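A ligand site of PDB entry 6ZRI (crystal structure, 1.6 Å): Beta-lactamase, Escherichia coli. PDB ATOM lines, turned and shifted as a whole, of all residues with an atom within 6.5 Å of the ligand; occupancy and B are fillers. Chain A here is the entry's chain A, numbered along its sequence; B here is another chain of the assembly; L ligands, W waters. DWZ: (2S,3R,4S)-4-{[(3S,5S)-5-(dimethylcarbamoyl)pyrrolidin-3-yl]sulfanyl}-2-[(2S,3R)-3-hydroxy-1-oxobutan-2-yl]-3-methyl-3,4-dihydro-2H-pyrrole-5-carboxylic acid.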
ATOM      1  N   PRO A  45     -15.922   7.433 -15.094  1.00  0.00           N
ATOM      2  CA  PRO A  45     -15.697   6.053 -14.627  1.00  0.00           C
ATOM      3  C   PRO A  45     -16.895   5.428 -13.939  1.00  0.00           C
ATOM      4  O   PRO A  45     -17.003   4.187 -13.918  1.00  0.00           O
ATOM      5  CB  PRO A  45     -14.508   6.157 -13.652  1.00  0.00           C
ATOM      6  CG  PRO A  45     -14.536   7.600 -13.220  1.00  0.00           C
ATOM      7  CD  PRO A  45     -15.089   8.410 -14.370  1.00  0.00           C
ATOM      8  N   ALA A  46     -17.801   6.243 -13.397  1.00  0.00           N
ATOM      9  CA  ALA A  46     -18.957   5.768 -12.621  1.00  0.00           C
ATOM     10  C   ALA A  46     -18.479   4.706 -11.609  1.00  0.00           C
ATOM     11  O   ALA A  46     -17.441   4.898 -10.993  1.00  0.00           O
ATOM     12  CB  ALA A  46     -20.038   5.202 -13.546  1.00  0.00           C
ATOM     13  N   SER A  47     -19.190   3.574 -11.509  1.00  0.00           N
ATOM     14  CA  SER A  47     -18.931   2.624 -10.429  1.00  0.00           C
ATOM     15  C   SER A  47     -17.559   1.956 -10.561  1.00  0.00           C
ATOM     16  O   SER A  47     -17.092   1.378  -9.570  1.00  0.00           O
ATOM     17  CB  SER A  47     -20.023   1.551 -10.337  1.00  0.00           C
ATOM     18  OG  SER A  47     -21.298   2.085  -9.994  1.00  0.00           O
ATOM     19  N   THR A  48     -16.892   2.014 -11.703  1.00  0.00           N
ATOM     20  CA  THR A  48     -15.538   1.490 -11.789  1.00  0.00           C
ATOM     21  C   THR A  48     -14.594   2.265 -10.868  1.00  0.00           C
ATOM     22  O   THR A  48     -13.546   1.747 -10.526  1.00  0.00           O
ATOM     23  CB  THR A  48     -14.964   1.385 -13.190  1.00  0.00           C
ATOM     24  OG1 THR A  48     -14.733   2.712 -13.705  1.00  0.00           O
ATOM     25  CG2 THR A  48     -15.892   0.611 -14.136  1.00  0.00           C
ATOM     26  N   KCX A  50     -15.007   2.656  -7.904  1.00  0.00           N
ATOM     27  CA  KCX A  50     -14.916   2.011  -6.588  1.00  0.00           C
ATOM     28  CB  KCX A  50     -16.105   1.092  -6.391  1.00  0.00           C
ATOM     29  CG  KCX A  50     -17.395   1.865  -6.104  1.00  0.00           C
ATOM     30  CD  KCX A  50     -18.699   1.051  -5.988  1.00  0.00           C
ATOM     31  CE  KCX A  50     -19.824   2.042  -5.667  1.00  0.00           C
ATOM     32  NZ  KCX A  50     -20.217   2.839  -6.853  1.00  0.00           N
ATOM     33  C   KCX A  50     -13.595   1.254  -6.422  1.00  0.00           C
ATOM     34  O   KCX A  50     -13.208   0.938  -5.293  1.00  0.00           O
ATOM     35  CX  KCX A  50     -19.879   4.169  -7.034  1.00  0.00           C
ATOM     36  OQ1 KCX A  50     -19.204   4.687  -6.028  1.00  0.00           O
ATOM     37  OQ2 KCX A  50     -20.121   4.781  -8.050  1.00  0.00           O
ATOM     38  N   MET A  79     -31.297   2.157  -4.273  1.00  0.00           N
ATOM     39  CA  MET A  79     -31.559   0.775  -4.695  1.00  0.00           C
ATOM     40  C   MET A  79     -31.805  -0.086  -3.454  1.00  0.00           C
ATOM     41  O   MET A  79     -31.108   0.041  -2.456  1.00  0.00           O
ATOM     42  CB  MET A  79     -30.368   0.134  -5.448  1.00  0.00           C
ATOM     43  CG  MET A  79     -29.783   0.961  -6.562  1.00  0.00           C
ATOM     44  SD  MET A  79     -30.881   1.022  -8.012  1.00  0.00           S
ATOM     45  CE  MET A  79     -30.481  -0.529  -8.816  1.00  0.00           C
ATOM     46  N   GLN A  81     -31.014  -3.140  -3.042  1.00  0.00           N
ATOM     47  CA  GLN A  81     -29.783  -3.917  -2.882  1.00  0.00           C
ATOM     48  C   GLN A  81     -28.803  -3.216  -1.936  1.00  0.00           C
ATOM     49  O   GLN A  81     -27.959  -3.858  -1.324  1.00  0.00           O
ATOM     50  CB  GLN A  81     -29.100  -4.132  -4.248  1.00  0.00           C
ATOM     51  CG  GLN A  81     -29.930  -4.902  -5.277  1.00  0.00           C
ATOM     52  CD  GLN A  81     -30.614  -4.118  -6.376  1.00  0.00           C
ATOM     53  OE1 GLN A  81     -30.786  -4.599  -7.496  1.00  0.00           O
ATOM     54  NE2 GLN A  81     -31.045  -2.892  -6.075  1.00  0.00           N
ATOM     55  N   TRP A  82     -28.907  -1.887  -1.775  1.00  0.00           N
ATOM     56  CA  TRP A  82     -28.032  -1.146  -0.887  1.00  0.00           C
ATOM     57  C   TRP A  82     -28.589  -1.006   0.537  1.00  0.00           C
ATOM     58  O   TRP A  82     -27.913  -0.484   1.405  1.00  0.00           O
ATOM     59  CB  TRP A  82     -27.724   0.227  -1.476  1.00  0.00           C
ATOM     60  CG  TRP A  82     -27.230   0.204  -2.881  1.00  0.00           C
ATOM     61  CD1 TRP A  82     -26.600  -0.793  -3.562  1.00  0.00           C
ATOM     62  CD2 TRP A  82     -27.223   1.339  -3.752  1.00  0.00           C
ATOM     63  NE1 TRP A  82     -26.209  -0.367  -4.800  1.00  0.00           N
ATOM     64  CE2 TRP A  82     -26.588   0.941  -4.950  1.00  0.00           C
ATOM     65  CE3 TRP A  82     -27.690   2.644  -3.614  1.00  0.00           C
ATOM     66  CZ2 TRP A  82     -26.438   1.805  -6.042  1.00  0.00           C
ATOM     67  CZ3 TRP A  82     -27.516   3.496  -4.674  1.00  0.00           C
ATOM     68  CH2 TRP A  82     -26.929   3.080  -5.870  1.00  0.00           C
ATOM     69  N   GLN A  93     -19.326  -5.067  -4.950  1.00  0.00           N
ATOM     70  CA  GLN A  93     -19.948  -5.930  -5.936  1.00  0.00           C
ATOM     71  C   GLN A  93     -21.404  -5.530  -6.186  1.00  0.00           C
ATOM     72  O   GLN A  93     -21.864  -5.771  -7.299  1.00  0.00           O
ATOM     73  CB  GLN A  93     -19.971  -7.351  -5.378  1.00  0.00           C
ATOM     74  CG  GLN A  93     -18.581  -7.959  -5.309  1.00  0.00           C
ATOM     75  CD  GLN A  93     -18.201  -8.794  -6.517  1.00  0.00           C
ATOM     76  OE1 GLN A  93     -19.075  -9.296  -7.218  1.00  0.00           O
ATOM     77  NE2 GLN A  93     -16.909  -8.994  -6.729  1.00  0.00           N
ATOM     78  N   VAL A  94     -22.067  -4.859  -5.238  1.00  0.00           N
ATOM     79  CA  VAL A  94     -23.430  -4.362  -5.500  1.00  0.00           C
ATOM     80  C   VAL A  94     -23.405  -2.880  -5.881  1.00  0.00           C
ATOM     81  O   VAL A  94     -24.451  -2.261  -5.976  1.00  0.00           O
ATOM     82  CB  VAL A  94     -24.456  -4.606  -4.367  1.00  0.00           C
ATOM     83  CG1 VAL A  94     -24.527  -6.115  -4.014  1.00  0.00           C
ATOM     84  CG2 VAL A  94     -24.163  -3.751  -3.112  1.00  0.00           C
ATOM     85  N   SER A  95     -22.200  -2.335  -6.011  1.00  0.00           N
ATOM     86  CA  SER A  95     -21.977  -0.917  -6.370  1.00  0.00           C
ATOM     87  C   SER A  95     -22.693   0.036  -5.422  1.00  0.00           C
ATOM     88  O   SER A  95     -23.372   0.928  -5.937  1.00  0.00           O
ATOM     89  CB  SER A  95     -22.395  -0.616  -7.806  1.00  0.00           C
ATOM     90  OG  SER A  95     -21.580  -1.332  -8.730  1.00  0.00           O
ATOM     91  N   ALA A  96     -22.517  -0.105  -4.098  1.00  0.00           N
ATOM     92  CA  ALA A  96     -23.277   0.682  -3.117  1.00  0.00           C
ATOM     93  C   ALA A  96     -22.703   2.113  -2.990  1.00  0.00           C
ATOM     94  O   ALA A  96     -21.847   2.375  -2.145  1.00  0.00           O
ATOM     95  CB  ALA A  96     -23.262  -0.024  -1.766  1.00  0.00           C
ATOM     96  N   VAL A  97     -23.124   2.991  -3.901  1.00  0.00           N
ATOM     97  CA  VAL A  97     -22.545   4.328  -3.991  1.00  0.00           C
ATOM     98  C   VAL A  97     -22.599   5.081  -2.657  1.00  0.00           C
ATOM     99  O   VAL A  97     -21.630   5.779  -2.332  1.00  0.00           O
ATOM    100  CB  VAL A  97     -23.158   5.136  -5.160  1.00  0.00           C
ATOM    101  CG1 VAL A  97     -24.636   5.406  -4.974  1.00  0.00           C
ATOM    102  CG2 VAL A  97     -22.476   6.490  -5.401  1.00  0.00           C
ATOM    103  N   TRP A 134     -16.862  11.349  -9.695  1.00  0.00           N
ATOM    104  CA  TRP A 134     -16.810  10.207 -10.596  1.00  0.00           C
ATOM    105  C   TRP A 134     -18.197   9.826 -11.096  1.00  0.00           C
ATOM    106  O   TRP A 134     -18.298   8.887 -11.911  1.00  0.00           O
ATOM    107  CB  TRP A 134     -16.183   8.962  -9.879  1.00  0.00           C
ATOM    108  CG  TRP A 134     -17.005   8.443  -8.760  1.00  0.00           C
ATOM    109  CD1 TRP A 134     -17.863   7.367  -8.826  1.00  0.00           C
ATOM    110  CD2 TRP A 134     -17.062   8.891  -7.384  1.00  0.00           C
ATOM    111  NE1 TRP A 134     -18.465   7.137  -7.617  1.00  0.00           N
ATOM    112  CE2 TRP A 134     -17.984   8.053  -6.708  1.00  0.00           C
ATOM    113  CE3 TRP A 134     -16.411   9.899  -6.648  1.00  0.00           C
ATOM    114  CZ2 TRP A 134     -18.264   8.174  -5.335  1.00  0.00           C
ATOM    115  CZ3 TRP A 134     -16.688  10.028  -5.280  1.00  0.00           C
ATOM    116  CH2 TRP A 134     -17.624   9.200  -4.635  1.00  0.00           C
ATOM    117  N   LEU A 135     -19.251  10.525 -10.636  1.00  0.00           N
ATOM    118  CA  LEU A 135     -20.635  10.212 -10.951  1.00  0.00           C
ATOM    119  C   LEU A 135     -21.210  11.259 -11.911  1.00  0.00           C
ATOM    120  O   LEU A 135     -21.986  10.918 -12.803  1.00  0.00           O
ATOM    121  CB  LEU A 135     -21.469  10.230  -9.671  1.00  0.00           C
ATOM    122  CG  LEU A 135     -21.037   9.142  -8.686  1.00  0.00           C
ATOM    123  CD1 LEU A 135     -21.645   9.360  -7.326  1.00  0.00           C
ATOM    124  CD2 LEU A 135     -21.383   7.777  -9.275  1.00  0.00           C
ATOM    125  N   LYS A 185     -15.316  -5.475 -12.698  1.00  0.00           N
ATOM    126  CA  LYS A 185     -16.204  -4.477 -12.126  1.00  0.00           C
ATOM    127  C   LYS A 185     -16.990  -3.796 -13.246  1.00  0.00           C
ATOM    128  O   LYS A 185     -16.367  -3.367 -14.205  1.00  0.00           O
ATOM    129  CB  LYS A 185     -15.320  -3.417 -11.439  1.00  0.00           C
ATOM    130  CG  LYS A 185     -16.112  -2.288 -10.757  1.00  0.00           C
ATOM    131  CD  LYS A 185     -16.704  -2.865  -9.463  1.00  0.00           C
ATOM    132  CE  LYS A 185     -17.776  -1.948  -8.874  1.00  0.00           C
ATOM    133  NZ  LYS A 185     -19.030  -1.976  -9.690  1.00  0.00           N
ATOM    134  N   THR A 186     -18.301  -3.681 -13.071  1.00  0.00           N
ATOM    135  CA  THR A 186     -19.121  -2.962 -14.031  1.00  0.00           C
ATOM    136  C   THR A 186     -19.258  -1.488 -13.652  1.00  0.00           C
ATOM    137  O   THR A 186     -19.014  -1.068 -12.505  1.00  0.00           O
ATOM    138  CB  THR A 186     -20.554  -3.509 -13.997  1.00  0.00           C
ATOM    139  OG1 THR A 186     -21.042  -3.535 -12.655  1.00  0.00           O
ATOM    140  CG2 THR A 186     -20.618  -4.923 -14.530  1.00  0.00           C
ATOM    141  N   GLY A 187     -19.760  -0.702 -14.628  1.00  0.00           N
ATOM    142  CA  GLY A 187     -20.212   0.638 -14.308  1.00  0.00           C
ATOM    143  C   GLY A 187     -21.366   0.999 -15.232  1.00  0.00           C
ATOM    144  O   GLY A 187     -21.436   0.505 -16.349  1.00  0.00           O
ATOM    145  N   TRP A 188     -22.203   1.931 -14.776  1.00  0.00           N
ATOM    146  CA  TRP A 188     -23.226   2.561 -15.614  1.00  0.00           C
ATOM    147  C   TRP A 188     -23.288   4.002 -15.167  1.00  0.00           C
ATOM    148  O   TRP A 188     -23.785   4.249 -14.065  1.00  0.00           O
ATOM    149  CB  TRP A 188     -24.562   1.886 -15.361  1.00  0.00           C
ATOM    150  CG  TRP A 188     -25.714   2.529 -16.091  1.00  0.00           C
ATOM    151  CD1 TRP A 188     -25.642   3.389 -17.163  1.00  0.00           C
ATOM    152  CD2 TRP A 188     -27.105   2.314 -15.827  1.00  0.00           C
ATOM    153  NE1 TRP A 188     -26.920   3.699 -17.579  1.00  0.00           N
ATOM    154  CE2 TRP A 188     -27.824   3.109 -16.749  1.00  0.00           C
ATOM    155  CE3 TRP A 188     -27.806   1.548 -14.872  1.00  0.00           C
ATOM    156  CZ2 TRP A 188     -29.230   3.112 -16.784  1.00  0.00           C
ATOM    157  CZ3 TRP A 188     -29.189   1.571 -14.885  1.00  0.00           C
ATOM    158  CH2 TRP A 188     -29.881   2.341 -15.827  1.00  0.00           C
ATOM    159  N   GLY A 189     -22.805   4.903 -16.021  1.00  0.00           N
ATOM    160  CA  GLY A 189     -22.802   6.333 -15.679  1.00  0.00           C
ATOM    161  C   GLY A 189     -24.004   7.021 -16.341  1.00  0.00           C
ATOM    162  O   GLY A 189     -23.946   7.237 -17.535  1.00  0.00           O
ATOM    163  N   MET A 190     -25.043   7.307 -15.543  1.00  0.00           N
ATOM    164  CA  MET A 190     -26.251   7.956 -16.029  1.00  0.00           C
ATOM    165  C   MET A 190     -26.118   9.466 -15.898  1.00  0.00           C
ATOM    166  O   MET A 190     -26.916  10.220 -16.456  1.00  0.00           O
ATOM    167  CB  MET A 190     -27.459   7.573 -15.156  1.00  0.00           C
ATOM    168  CG  MET A 190     -27.880   6.140 -15.253  1.00  0.00           C
ATOM    169  SD  MET A 190     -28.119   5.734 -13.524  1.00  0.00           S
ATOM    170  CE  MET A 190     -26.686   6.607 -12.858  1.00  0.00           C
ATOM    171  N   LEU A 224     -28.174  -2.698 -21.105  1.00  0.00           N
ATOM    172  CA  LEU A 224     -27.131  -2.811 -20.080  1.00  0.00           C
ATOM    173  C   LEU A 224     -26.392  -4.166 -20.099  1.00  0.00           C
ATOM    174  O   LEU A 224     -25.195  -4.235 -19.860  1.00  0.00           O
ATOM    175  CB  LEU A 224     -27.793  -2.568 -18.735  1.00  0.00           C
ATOM    176  CG  LEU A 224     -26.899  -2.039 -17.626  1.00  0.00           C
ATOM    177  CD1 LEU A 224     -26.206  -0.742 -18.049  1.00  0.00           C
ATOM    178  CD2 LEU A 224     -27.707  -1.863 -16.348  1.00  0.00           C
ATOM    179  N   ARG A 227     -22.881  -4.859 -21.787  1.00  0.00           N
ATOM    180  CA  ARG A 227     -21.587  -4.375 -21.306  1.00  0.00           C
ATOM    181  C   ARG A 227     -20.749  -5.552 -20.807  1.00  0.00           C
ATOM    182  O   ARG A 227     -19.520  -5.421 -20.795  1.00  0.00           O
ATOM    183  CB  ARG A 227     -21.742  -3.256 -20.260  1.00  0.00           C
ATOM    184  CG  ARG A 227     -22.151  -3.826 -18.908  1.00  0.00           C
ATOM    185  CD  ARG A 227     -22.617  -2.785 -17.913  1.00  0.00           C
ATOM    186  NE  ARG A 227     -23.265  -3.475 -16.807  1.00  0.00           N
ATOM    187  CZ  ARG A 227     -23.626  -2.918 -15.649  1.00  0.00           C
ATOM    188  NH1 ARG A 227     -23.415  -1.633 -15.425  1.00  0.00           N
ATOM    189  NH2 ARG A 227     -24.220  -3.661 -14.728  1.00  0.00           N
ATOM    190  N   PRO B 178     -21.995 -11.756  -5.600  1.00  0.00           N
ATOM    191  CA  PRO B 178     -21.735 -10.436  -5.012  1.00  0.00           C
ATOM    192  C   PRO B 178     -21.782 -10.450  -3.496  1.00  0.00           C
ATOM    193  O   PRO B 178     -20.944  -9.791  -2.867  1.00  0.00           O
ATOM    194  CB  PRO B 178     -22.893  -9.612  -5.624  1.00  0.00           C
ATOM    195  CG  PRO B 178     -22.967 -10.187  -7.015  1.00  0.00           C
ATOM    196  CD  PRO B 178     -22.834 -11.692  -6.810  1.00  0.00           C
ATOM    197  N   GLU B 179     -22.705 -11.222  -2.891  1.00  0.00           N
ATOM    198  CA  GLU B 179     -22.729 -11.260  -1.432  1.00  0.00           C
ATOM    199  C   GLU B 179     -22.567 -12.684  -0.918  1.00  0.00           C
ATOM    200  O   GLU B 179     -23.184 -13.046   0.066  1.00  0.00           O
ATOM    201  CB  GLU B 179     -24.030 -10.669  -0.882  1.00  0.00           C
ATOM    202  CG  GLU B 179     -24.080  -9.160  -1.070  1.00  0.00           C
ATOM    203  CD  GLU B 179     -25.486  -8.628  -0.841  1.00  0.00           C
ATOM    204  OE1 GLU B 179     -25.815  -8.324   0.309  1.00  0.00           O
ATOM    205  OE2 GLU B 179     -26.264  -8.709  -1.768  1.00  0.00           O
HETATM  206  CBE DWZ L   1     -24.679  -7.302  -7.929  1.00  0.00           C
HETATM  207  NBC DWZ L   1     -25.452  -6.338  -8.722  1.00  0.00           N
HETATM  208  CBD DWZ L   1     -25.147  -6.267 -10.158  1.00  0.00           C
HETATM  209  C   DWZ L   1     -26.406  -5.573  -8.167  1.00  0.00           C
HETATM  210  O   DWZ L   1     -26.795  -5.711  -6.997  1.00  0.00           O
HETATM  211  CA  DWZ L   1     -27.001  -4.498  -9.084  1.00  0.00           C
HETATM  212  CB  DWZ L   1     -26.072  -3.263  -9.171  1.00  0.00           C
HETATM  213  N   DWZ L   1     -28.268  -3.969  -8.529  1.00  0.00           N
HETATM  214  CD  DWZ L   1     -28.019  -2.611  -8.004  1.00  0.00           C
HETATM  215  CG  DWZ L   1     -27.063  -2.109  -9.070  1.00  0.00           C
HETATM  216  SAK DWZ L   1     -26.344  -0.465  -8.783  1.00  0.00           S
HETATM  217  CAI DWZ L   1     -26.253   0.321 -10.465  1.00  0.00           C
HETATM  218  CAH DWZ L   1     -25.803   1.759 -10.202  1.00  0.00           C
HETATM  219  CAS DWZ L   1     -26.352   2.699 -11.260  1.00  0.00           C
HETATM  220  CAL DWZ L   1     -25.184  -0.144 -11.457  1.00  0.00           C
HETATM  221  CAM DWZ L   1     -25.387  -1.200 -12.526  1.00  0.00           C
HETATM  222  OAT DWZ L   1     -26.551  -1.581 -12.757  1.00  0.00           O
HETATM  223  OAU DWZ L   1     -24.379  -1.743 -12.996  1.00  0.00           O
HETATM  224  NAJ DWZ L   1     -24.038   0.448 -11.250  1.00  0.00           N
HETATM  225  CAD DWZ L   1     -24.282   1.552 -10.275  1.00  0.00           C
HETATM  226  CAB DWZ L   1     -23.529   2.809 -10.684  1.00  0.00           C
HETATM  227  CAE DWZ L   1     -23.529   3.968  -9.676  1.00  0.00           C
HETATM  228  CAF DWZ L   1     -23.345   3.504  -8.272  1.00  0.00           C
HETATM  229  OAG DWZ L   1     -22.401   4.820 -10.018  1.00  0.00           O
HETATM  230  CAA DWZ L   1     -22.099   2.378 -11.011  1.00  0.00           C
HETATM  231  OAC DWZ L   1     -21.647   2.541 -12.129  1.00  0.00           O
HETATM  232  O   HOH W   1     -29.236  -1.981 -12.525  1.00  0.00           O
HETATM  233  O   HOH W   2     -23.137   6.177 -12.079  1.00  0.00           O
HETATM  234  O   HOH W   3     -26.343  -4.750 -13.101  1.00  0.00           O
HETATM  235  O   HOH W   4     -21.969  -1.135 -11.586  1.00  0.00           O
HETATM  236  O   HOH W   5     -23.231  -4.265 -11.827  1.00  0.00           O
HETATM  237  O   HOH W   6     -30.071  -3.934 -10.521  1.00  0.00           O
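The backbone carbonyl oxygen of Trp 134 lies within hydrogen-bond range of the backbone NH of Ala 46, at 3.1 Å. OQ2 of KCX 50 lies within hydrogen-bond range of the indole nitrogen (NE1) of Trp 134, at 2.9 Å. NZ of KCX 50 sits at hydrogen-bond distance from OG of Ser 47 (3.4 Å). OG of Ser 95 is in hydrogen-bond range of NZ of Lys 185 (2.8 Å). NH1 of Arg 227 sits at hydrogen-bond distance from O of Gly 187, at 3.1 Å. The indole nitrogen of Trp 82 is in hydrogen-bond range of the backbone carbonyl oxygen of Val 94. The indole nitrogen of Trp 82 lies close to the backbone carbonyl oxygen of Ser 95, 3.3 Å away.
An oxygen (OAU) of the ligand is in salt-bridge range of the guanidinium group of Arg 227, 2.6 Å away. A carbon (CAA) of the ligand is covalently linked to the side-chain hydroxyl (OG) of Ser 47 (1.3 Å). OQ2 of KCX 50 lies within hydrogen-bond range of an oxygen (OAG) of the ligand (3.0 Å). OAC of the ligand sits at hydrogen-bond distance from N of Trp 188 (2.8 Å). N of Ser 47 lies close to OAC of the ligand (2.7 Å). N of the ligand lies within hydrogen-bond range of OE1 of Gln 81 (2.8 Å).
Water W2 lies within hydrogen-bond range of an oxygen (OAG) of the ligand (2.6 Å) and the backbone carbonyl oxygen of Trp 188 (2.8 Å). Water W4 lies within hydrogen-bond range of NAJ of the ligand (2.6 Å), OG1 of Thr 186 (2.8 Å) and OG of Ser 95 (2.9 Å). Water W6 bridges N of the ligand (2.7 Å) and OE1 of Gln 81 (3.2 Å). Water W5 lies within hydrogen-bond range of the side-chain hydroxyl (OG1) of Thr 186, an oxygen (OAU) of the ligand and the guanidinium group (NH2) of Arg 227. Water W3 bridges the guanidinium group (NH2) of Arg 227 (2.9 Å) and an oxygen (OAT) of the ligand (3.2 Å).
Merely in contact with the ligand: Ala 46 (3.4 Å), Met 79 (3.3 Å), Trp 82 (3.6 Å), Gln 93 (3.3 Å), Val 94 (3.7 Å), Ser 95 (3.5 Å), Val 97 (3.5 Å), Leu 135 (3.2 Å), Thr 186 (3.8 Å), Gly 187 (3.2 Å), Leu 224 (3.8 Å) and Pro 178 of chain B (3.5 Å). Hydrophobic or aromatic side chains within 4 Å of the ligand: Ala 46, Met 79, Trp 82, Val 94, Val 97, Leu 135, Trp 188, Leu 224 and Pro 178 of chain B. 17 residues have an atom within 4 Å of the ligand: Ala 46, Ser 47, KCX 50, Met 79, Gln 81, Trp 82, Gln 93, Val 94, Ser 95, Val 97, Leu 135, Thr 186, Gly 187, Trp 188, Leu 224, Arg 227 and Pro 178 of chain B.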
